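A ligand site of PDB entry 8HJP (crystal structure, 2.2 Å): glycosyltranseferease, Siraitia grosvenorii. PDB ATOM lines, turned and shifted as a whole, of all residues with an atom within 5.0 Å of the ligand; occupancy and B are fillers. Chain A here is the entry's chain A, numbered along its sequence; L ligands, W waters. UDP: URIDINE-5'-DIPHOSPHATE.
NE2 of Gln 335 is in hydrogen-bond range of OG of Ser 355 (3.1 Å).
NE2 of Gln 335 is in hydrogen-bond range of OE1 of Glu 358.
The backbone carbonyl oxygen of Gly 21 is in hydrogen-bond range of the side-chain amide nitrogen of Asn 354 (3.1 Å).
A ring nitrogen (NE2) of His 350 lies close to the backbone NH (N) of Gly 352.
The backbone NH of His 350 lies within hydrogen-bond range of the backbone carbonyl oxygen of Ser 269, at 3.3 Å.
OH of Tyr 20 lies within hydrogen-bond range of NZ of Lys 55, at 2.9 Å.
N of Gly 271 is in hydrogen-bond range of OG of Ser 269, at 3.2 Å.
An oxygen (O2A) of the ligand is in hydrogen-bond range of the backbone NH (N) of Ser 355, 2.7 Å away.
An oxygen (O2A) of the ligand is in hydrogen-bond range of the side-chain hydroxyl (OG) of Ser 355 (2.6 Å).
The side-chain carboxylate (OE1) of Glu 358 sits at hydrogen-bond distance from an oxygen (O2') of the ligand, 2.6 Å away.
An oxygen (O3B) of the ligand is in hydrogen-bond range of the backbone NH (N) of Ser 272 (3.0 Å).
An oxygen (O3B) of the ligand is in hydrogen-bond range of the side-chain hydroxyl (OG) of Ser 272 (2.7 Å).
The backbone NH (N) of Ala 333 lies within hydrogen-bond range of an oxygen (O4) of the ligand, 3.1 Å away.
O of Ala 333 is in hydrogen-bond range of N3 of the ligand, 2.8 Å away.
An oxygen (O1A) of the ligand lies within hydrogen-bond range of the backbone NH of Asn 354 (3.0 Å).
The side-chain amide nitrogen (ND2) of Asn 354 sits at hydrogen-bond distance from an oxygen (O1A) of the ligand.
An oxygen (O2') of the ligand is in hydrogen-bond range of the side-chain amide nitrogen of Gln 335 (3.0 Å).
NE2 of His 350 sits at hydrogen-bond distance from O3A of the ligand (3.1 Å).
An oxygen (O1A) of the ligand is in hydrogen-bond range of the backbone NH (N) of Trp 353.
Water W2 lies within hydrogen-bond range of O1B of the ligand, N of Gly 21 and OE2 of Glu 273.
Water W5 lies within hydrogen-bond range of an oxygen (O2) of the ligand (2.9 Å) and the indole nitrogen of Trp 332 (3.1 Å).
Water W4 bridges the backbone NH of Ala 336 (3.0 Å) and an oxygen (O2) of the ligand (3.1 Å).
Water W3 lies within hydrogen-bond range of the backbone NH of Glu 273 (2.8 Å), an oxygen (O2B) of the ligand (3.3 Å) and the backbone NH of Ser 272 (3.4 Å).
Water W6 lies within hydrogen-bond range of the side-chain amide oxygen (OE1) of Gln 335, the side-chain hydroxyl (OG) of Ser 269 and the side-chain hydroxyl (OG) of Ser 355.
An oxygen (O2A) of the ligand lies close to the backbone carbonyl oxygen (O) of Gly 352.
Residues that only touch the ligand: Trp 332, Tyr 20, Gly 21, Val 298 and Gly 271.
Hydrophobic or aromatic side chains within 4 Å of the ligand: Tyr 20, Val 298, Trp 332, Ala 333 and His 350.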
ATOM      1  N   TYR A  20     -31.482 -26.368  13.513  1.00  0.00           N
ATOM      2  CA  TYR A  20     -30.261 -26.335  14.302  1.00  0.00           C
ATOM      3  C   TYR A  20     -30.319 -25.275  15.402  1.00  0.00           C
ATOM      4  O   TYR A  20     -29.881 -25.524  16.530  1.00  0.00           O
ATOM      5  CB  TYR A  20     -29.056 -26.097  13.401  1.00  0.00           C
ATOM      6  CG  TYR A  20     -27.754 -26.251  14.133  1.00  0.00           C
ATOM      7  CD1 TYR A  20     -27.183 -27.499  14.314  1.00  0.00           C
ATOM      8  CD2 TYR A  20     -27.097 -25.147  14.666  1.00  0.00           C
ATOM      9  CE1 TYR A  20     -25.997 -27.646  15.000  1.00  0.00           C
ATOM     10  CE2 TYR A  20     -25.915 -25.282  15.345  1.00  0.00           C
ATOM     11  CZ  TYR A  20     -25.368 -26.537  15.511  1.00  0.00           C
ATOM     12  OH  TYR A  20     -24.173 -26.670  16.187  1.00  0.00           O
ATOM     13  N   GLY A  21     -30.843 -24.084  15.097  1.00  0.00           N
ATOM     14  CA  GLY A  21     -30.937 -23.054  16.114  1.00  0.00           C
ATOM     15  C   GLY A  21     -31.809 -23.457  17.294  1.00  0.00           C
ATOM     16  O   GLY A  21     -31.479 -23.183  18.445  1.00  0.00           O
ATOM     17  N   SER A  24     -29.846 -26.100  19.298  1.00  0.00           N
ATOM     18  CA  SER A  24     -28.775 -25.520  20.102  1.00  0.00           C
ATOM     19  C   SER A  24     -29.321 -24.853  21.358  1.00  0.00           C
ATOM     20  O   SER A  24     -28.788 -25.023  22.453  1.00  0.00           O
ATOM     21  CB  SER A  24     -27.956 -24.534  19.286  1.00  0.00           C
ATOM     22  OG  SER A  24     -27.019 -23.853  20.109  1.00  0.00           O
ATOM     23  N   LYS A  55     -21.482 -30.719  20.789  1.00  0.00           N
ATOM     24  CA  LYS A  55     -21.579 -29.642  21.770  1.00  0.00           C
ATOM     25  C   LYS A  55     -21.925 -30.132  23.170  1.00  0.00           C
ATOM     26  O   LYS A  55     -21.939 -29.319  24.102  1.00  0.00           O
ATOM     27  CB  LYS A  55     -22.602 -28.607  21.318  1.00  0.00           C
ATOM     28  CG  LYS A  55     -22.359 -28.100  19.899  1.00  0.00           C
ATOM     29  CD  LYS A  55     -23.175 -26.853  19.589  1.00  0.00           C
ATOM     30  CE  LYS A  55     -22.377 -25.903  18.715  1.00  0.00           C
ATOM     31  NZ  LYS A  55     -23.214 -24.786  18.181  1.00  0.00           N
ATOM     32  N   PHE A 267     -17.841 -11.498   9.137  1.00  0.00           N
ATOM     33  CA  PHE A 267     -18.324 -12.856   8.919  1.00  0.00           C
ATOM     34  C   PHE A 267     -19.647 -12.741   8.189  1.00  0.00           C
ATOM     35  O   PHE A 267     -20.488 -11.912   8.541  1.00  0.00           O
ATOM     36  CB  PHE A 267     -18.482 -13.568  10.257  1.00  0.00           C
ATOM     37  CG  PHE A 267     -18.989 -14.976  10.150  1.00  0.00           C
ATOM     38  CD1 PHE A 267     -18.269 -15.940   9.463  1.00  0.00           C
ATOM     39  CD2 PHE A 267     -20.167 -15.358  10.770  1.00  0.00           C
ATOM     40  CE1 PHE A 267     -18.732 -17.244   9.372  1.00  0.00           C
ATOM     41  CE2 PHE A 267     -20.634 -16.644  10.682  1.00  0.00           C
ATOM     42  CZ  PHE A 267     -19.917 -17.597   9.989  1.00  0.00           C
ATOM     43  N   SER A 269     -22.968 -14.857   7.048  1.00  0.00           N
ATOM     44  CA  SER A 269     -23.794 -16.058   7.099  1.00  0.00           C
ATOM     45  C   SER A 269     -25.262 -15.710   7.006  1.00  0.00           C
ATOM     46  O   SER A 269     -25.704 -14.701   7.563  1.00  0.00           O
ATOM     47  CB  SER A 269     -23.576 -16.913   8.351  1.00  0.00           C
ATOM     48  OG  SER A 269     -24.409 -18.071   8.251  1.00  0.00           O
ATOM     49  N   GLY A 271     -27.552 -18.300   7.767  1.00  0.00           N
ATOM     50  CA  GLY A 271     -28.181 -19.295   8.598  1.00  0.00           C
ATOM     51  C   GLY A 271     -28.085 -20.724   8.089  1.00  0.00           C
ATOM     52  O   GLY A 271     -27.402 -21.052   7.122  1.00  0.00           O
ATOM     53  N   SER A 272     -28.795 -21.585   8.811  1.00  0.00           N
ATOM     54  CA  SER A 272     -28.832 -23.018   8.518  1.00  0.00           C
ATOM     55  C   SER A 272     -30.009 -23.438   7.639  1.00  0.00           C
ATOM     56  O   SER A 272     -30.016 -24.581   7.169  1.00  0.00           O
ATOM     57  CB  SER A 272     -28.878 -23.809   9.827  1.00  0.00           C
ATOM     58  OG  SER A 272     -30.128 -23.641  10.485  1.00  0.00           O
ATOM     59  N   GLU A 273     -30.984 -22.561   7.395  1.00  0.00           N
ATOM     60  CA  GLU A 273     -32.186 -22.955   6.678  1.00  0.00           C
ATOM     61  C   GLU A 273     -32.472 -22.166   5.402  1.00  0.00           C
ATOM     62  O   GLU A 273     -33.371 -22.567   4.649  1.00  0.00           O
ATOM     63  CB  GLU A 273     -33.421 -22.868   7.586  1.00  0.00           C
ATOM     64  CG  GLU A 273     -33.283 -23.593   8.915  1.00  0.00           C
ATOM     65  CD  GLU A 273     -34.525 -23.452   9.771  1.00  0.00           C
ATOM     66  OE1 GLU A 273     -35.395 -22.623   9.436  1.00  0.00           O
ATOM     67  OE2 GLU A 273     -34.633 -24.180  10.777  1.00  0.00           O
ATOM     68  N   VAL A 298     -19.741 -17.962   4.515  1.00  0.00           N
ATOM     69  CA  VAL A 298     -20.164 -19.354   4.434  1.00  0.00           C
ATOM     70  C   VAL A 298     -21.307 -19.439   3.434  1.00  0.00           C
ATOM     71  O   VAL A 298     -22.361 -18.819   3.619  1.00  0.00           O
ATOM     72  CB  VAL A 298     -20.560 -19.920   5.814  1.00  0.00           C
ATOM     73  CG1 VAL A 298     -21.545 -19.006   6.530  1.00  0.00           C
ATOM     74  CG2 VAL A 298     -21.137 -21.321   5.666  1.00  0.00           C
ATOM     75  N   GLY A 331     -20.385 -25.019   3.097  1.00  0.00           N
ATOM     76  CA  GLY A 331     -21.242 -25.802   3.978  1.00  0.00           C
ATOM     77  C   GLY A 331     -21.432 -25.297   5.392  1.00  0.00           C
ATOM     78  O   GLY A 331     -22.539 -24.882   5.756  1.00  0.00           O
ATOM     79  N   TRP A 332     -20.378 -25.329   6.205  1.00  0.00           N
ATOM     80  CA  TRP A 332     -20.496 -25.004   7.628  1.00  0.00           C
ATOM     81  C   TRP A 332     -19.191 -24.399   8.100  1.00  0.00           C
ATOM     82  O   TRP A 332     -18.106 -24.780   7.639  1.00  0.00           O
ATOM     83  CB  TRP A 332     -20.870 -26.256   8.431  1.00  0.00           C
ATOM     84  CG  TRP A 332     -21.380 -26.003   9.820  1.00  0.00           C
ATOM     85  CD1 TRP A 332     -20.665 -26.073  10.985  1.00  0.00           C
ATOM     86  CD2 TRP A 332     -22.715 -25.660  10.196  1.00  0.00           C
ATOM     87  NE1 TRP A 332     -21.476 -25.797  12.055  1.00  0.00           N
ATOM     88  CE2 TRP A 332     -22.741 -25.530  11.601  1.00  0.00           C
ATOM     89  CE3 TRP A 332     -23.899 -25.438   9.479  1.00  0.00           C
ATOM     90  CZ2 TRP A 332     -23.900 -25.207  12.299  1.00  0.00           C
ATOM     91  CZ3 TRP A 332     -25.045 -25.112  10.174  1.00  0.00           C
ATOM     92  CH2 TRP A 332     -25.041 -24.994  11.570  1.00  0.00           C
ATOM     93  N   ALA A 333     -19.286 -23.443   9.020  1.00  0.00           N
ATOM     94  CA  ALA A 333     -18.130 -22.753   9.556  1.00  0.00           C
ATOM     95  C   ALA A 333     -18.208 -22.682  11.070  1.00  0.00           C
ATOM     96  O   ALA A 333     -19.299 -22.755  11.645  1.00  0.00           O
ATOM     97  CB  ALA A 333     -18.038 -21.333   8.974  1.00  0.00           C
ATOM     98  N   GLN A 335     -18.779 -20.641  13.500  1.00  0.00           N
ATOM     99  CA  GLN A 335     -19.272 -19.268  13.596  1.00  0.00           C
ATOM    100  C   GLN A 335     -18.873 -18.610  14.906  1.00  0.00           C
ATOM    101  O   GLN A 335     -18.365 -17.483  14.915  1.00  0.00           O
ATOM    102  CB  GLN A 335     -20.792 -19.246  13.427  1.00  0.00           C
ATOM    103  CG  GLN A 335     -21.444 -17.960  13.880  1.00  0.00           C
ATOM    104  CD  GLN A 335     -22.852 -17.811  13.349  1.00  0.00           C
ATOM    105  OE1 GLN A 335     -23.151 -18.189  12.216  1.00  0.00           O
ATOM    106  NE2 GLN A 335     -23.738 -17.245  14.176  1.00  0.00           N
ATOM    107  N   ALA A 336     -19.101 -19.290  16.027  1.00  0.00           N
ATOM    108  CA  ALA A 336     -18.782 -18.697  17.325  1.00  0.00           C
ATOM    109  C   ALA A 336     -17.290 -18.390  17.443  1.00  0.00           C
ATOM    110  O   ALA A 336     -16.905 -17.339  17.971  1.00  0.00           O
ATOM    111  CB  ALA A 336     -19.237 -19.614  18.459  1.00  0.00           C
ATOM    112  N   HIS A 350     -28.183 -12.807   8.609  1.00  0.00           N
ATOM    113  CA  HIS A 350     -29.614 -12.819   8.355  1.00  0.00           C
ATOM    114  C   HIS A 350     -30.416 -12.434   9.582  1.00  0.00           C
ATOM    115  O   HIS A 350     -31.621 -12.239   9.482  1.00  0.00           O
ATOM    116  CB  HIS A 350     -30.058 -14.186   7.825  1.00  0.00           C
ATOM    117  CG  HIS A 350     -30.027 -15.257   8.865  1.00  0.00           C
ATOM    118  ND1 HIS A 350     -28.902 -15.557   9.610  1.00  0.00           N
ATOM    119  CD2 HIS A 350     -30.986 -16.124   9.277  1.00  0.00           C
ATOM    120  CE1 HIS A 350     -29.171 -16.550  10.438  1.00  0.00           C
ATOM    121  NE2 HIS A 350     -30.430 -16.917  10.255  1.00  0.00           N
ATOM    122  N   GLY A 352     -30.997 -14.271  12.337  1.00  0.00           N
ATOM    123  CA  GLY A 352     -31.634 -15.314  13.127  1.00  0.00           C
ATOM    124  C   GLY A 352     -31.258 -15.131  14.587  1.00  0.00           C
ATOM    125  O   GLY A 352     -30.153 -14.702  14.918  1.00  0.00           O
ATOM    126  N   TRP A 353     -32.222 -15.418  15.472  1.00  0.00           N
ATOM    127  CA  TRP A 353     -32.077 -15.080  16.889  1.00  0.00           C
ATOM    128  C   TRP A 353     -30.757 -15.532  17.496  1.00  0.00           C
ATOM    129  O   TRP A 353     -30.060 -14.738  18.139  1.00  0.00           O
ATOM    130  CB  TRP A 353     -33.244 -15.657  17.685  1.00  0.00           C
ATOM    131  CG  TRP A 353     -33.344 -15.071  19.043  1.00  0.00           C
ATOM    132  CD1 TRP A 353     -33.109 -15.707  20.229  1.00  0.00           C
ATOM    133  CD2 TRP A 353     -33.653 -13.705  19.383  1.00  0.00           C
ATOM    134  NE1 TRP A 353     -33.289 -14.842  21.280  1.00  0.00           N
ATOM    135  CE2 TRP A 353     -33.615 -13.605  20.785  1.00  0.00           C
ATOM    136  CE3 TRP A 353     -33.968 -12.571  18.634  1.00  0.00           C
ATOM    137  CZ2 TRP A 353     -33.872 -12.414  21.458  1.00  0.00           C
ATOM    138  CZ3 TRP A 353     -34.239 -11.387  19.301  1.00  0.00           C
ATOM    139  CH2 TRP A 353     -34.182 -11.320  20.695  1.00  0.00           C
ATOM    140  N   ASN A 354     -30.396 -16.814  17.320  1.00  0.00           N
ATOM    141  CA  ASN A 354     -29.162 -17.288  17.951  1.00  0.00           C
ATOM    142  C   ASN A 354     -27.942 -16.525  17.436  1.00  0.00           C
ATOM    143  O   ASN A 354     -27.050 -16.170  18.216  1.00  0.00           O
ATOM    144  CB  ASN A 354     -28.984 -18.787  17.736  1.00  0.00           C
ATOM    145  CG  ASN A 354     -30.018 -19.605  18.464  1.00  0.00           C
ATOM    146  OD1 ASN A 354     -29.996 -19.719  19.688  1.00  0.00           O
ATOM    147  ND2 ASN A 354     -30.933 -20.203  17.708  1.00  0.00           N
ATOM    148  N   SER A 355     -27.886 -16.257  16.129  1.00  0.00           N
ATOM    149  CA  SER A 355     -26.779 -15.478  15.585  1.00  0.00           C
ATOM    150  C   SER A 355     -26.767 -14.076  16.187  1.00  0.00           C
ATOM    151  O   SER A 355     -25.696 -13.526  16.501  1.00  0.00           O
ATOM    152  CB  SER A 355     -26.851 -15.424  14.068  1.00  0.00           C
ATOM    153  OG  SER A 355     -26.708 -16.702  13.504  1.00  0.00           O
ATOM    154  N   VAL A 356     -27.947 -13.479  16.355  1.00  0.00           N
ATOM    155  CA  VAL A 356     -28.023 -12.165  16.983  1.00  0.00           C
ATOM    156  C   VAL A 356     -27.531 -12.237  18.421  1.00  0.00           C
ATOM    157  O   VAL A 356     -26.757 -11.387  18.871  1.00  0.00           O
ATOM    158  CB  VAL A 356     -29.461 -11.612  16.899  1.00  0.00           C
ATOM    159  CG1 VAL A 356     -29.612 -10.375  17.774  1.00  0.00           C
ATOM    160  CG2 VAL A 356     -29.804 -11.270  15.464  1.00  0.00           C
ATOM    161  N   GLU A 358     -25.511 -14.476  19.733  1.00  0.00           N
ATOM    162  CA  GLU A 358     -24.076 -14.728  19.731  1.00  0.00           C
ATOM    163  C   GLU A 358     -23.297 -13.457  19.441  1.00  0.00           C
ATOM    164  O   GLU A 358     -22.294 -13.169  20.104  1.00  0.00           O
ATOM    165  CB  GLU A 358     -23.732 -15.827  18.719  1.00  0.00           C
ATOM    166  CG  GLU A 358     -24.164 -17.215  19.166  1.00  0.00           C
ATOM    167  CD  GLU A 358     -24.076 -18.241  18.066  1.00  0.00           C
ATOM    168  OE1 GLU A 358     -23.537 -17.907  16.981  1.00  0.00           O
ATOM    169  OE2 GLU A 358     -24.528 -19.385  18.278  1.00  0.00           O
ATOM    170  N   GLN A 375     -36.768 -12.621  11.279  1.00  0.00           N
ATOM    171  CA  GLN A 375     -35.507 -11.900  11.059  1.00  0.00           C
ATOM    172  C   GLN A 375     -35.692 -10.392  10.879  1.00  0.00           C
ATOM    173  O   GLN A 375     -34.891  -9.639  11.460  1.00  0.00           O
ATOM    174  CB  GLN A 375     -34.754 -12.542   9.889  1.00  0.00           C
ATOM    175  CG  GLN A 375     -34.453 -14.026  10.144  1.00  0.00           C
ATOM    176  CD  GLN A 375     -34.296 -14.834   8.880  1.00  0.00           C
ATOM    177  OE1 GLN A 375     -34.007 -14.299   7.808  1.00  0.00           O
ATOM    178  NE2 GLN A 375     -34.476 -16.146   8.987  1.00  0.00           N
HETATM  179  N1  UDP L   1     -24.040 -21.819  12.795  1.00  0.00           N
HETATM  180  C2  UDP L   1     -22.739 -22.283  12.813  1.00  0.00           C
HETATM  181  N3  UDP L   1     -22.099 -22.314  11.584  1.00  0.00           N
HETATM  182  C4  UDP L   1     -22.641 -21.923  10.378  1.00  0.00           C
HETATM  183  C5  UDP L   1     -23.990 -21.455  10.445  1.00  0.00           C
HETATM  184  C6  UDP L   1     -24.642 -21.418  11.627  1.00  0.00           C
HETATM  185  O2  UDP L   1     -22.170 -22.666  13.826  1.00  0.00           O
HETATM  186  O4  UDP L   1     -21.954 -21.994   9.349  1.00  0.00           O
HETATM  187  C1' UDP L   1     -24.811 -21.764  14.052  1.00  0.00           C
HETATM  188  C2' UDP L   1     -24.959 -20.310  14.611  1.00  0.00           C
HETATM  189  O2' UDP L   1     -23.848 -19.963  15.435  1.00  0.00           O
HETATM  190  C3' UDP L   1     -26.223 -20.431  15.420  1.00  0.00           C
HETATM  191  C4' UDP L   1     -27.056 -21.436  14.625  1.00  0.00           C
HETATM  192  O4' UDP L   1     -26.147 -22.209  13.795  1.00  0.00           O
HETATM  193  O3' UDP L   1     -25.928 -20.968  16.716  1.00  0.00           O
HETATM  194  C5' UDP L   1     -28.057 -20.748  13.741  1.00  0.00           C
HETATM  195  O5' UDP L   1     -29.179 -20.362  14.491  1.00  0.00           O
HETATM  196  PA  UDP L   1     -29.907 -18.930  14.137  1.00  0.00           P
HETATM  197  O1A UDP L   1     -31.039 -18.677  15.112  1.00  0.00           O
HETATM  198  O2A UDP L   1     -28.892 -17.824  14.218  1.00  0.00           O
HETATM  199  O3A UDP L   1     -30.568 -18.955  12.626  1.00  0.00           O
HETATM  200  PB  UDP L   1     -31.477 -20.077  11.825  1.00  0.00           P
HETATM  201  O1B UDP L   1     -32.393 -20.766  12.812  1.00  0.00           O
HETATM  202  O2B UDP L   1     -32.286 -19.397  10.748  1.00  0.00           O
HETATM  203  O3B UDP L   1     -30.558 -21.084  11.193  1.00  0.00           O
HETATM  204  O   HOH W   1     -33.727 -19.197  15.328  1.00  0.00           O
HETATM  205  O   HOH W   2     -32.802 -23.140  13.045  1.00  0.00           O
HETATM  206  O   HOH W   3     -31.347 -19.773   7.598  1.00  0.00           O
HETATM  207  O   HOH W   4     -20.669 -21.756  16.440  1.00  0.00           O
HETATM  208  O   HOH W   5     -20.326 -24.703  14.739  1.00  0.00           O
HETATM  209  O   HOH W   6     -25.410 -18.186  10.934  1.00  0.00           O
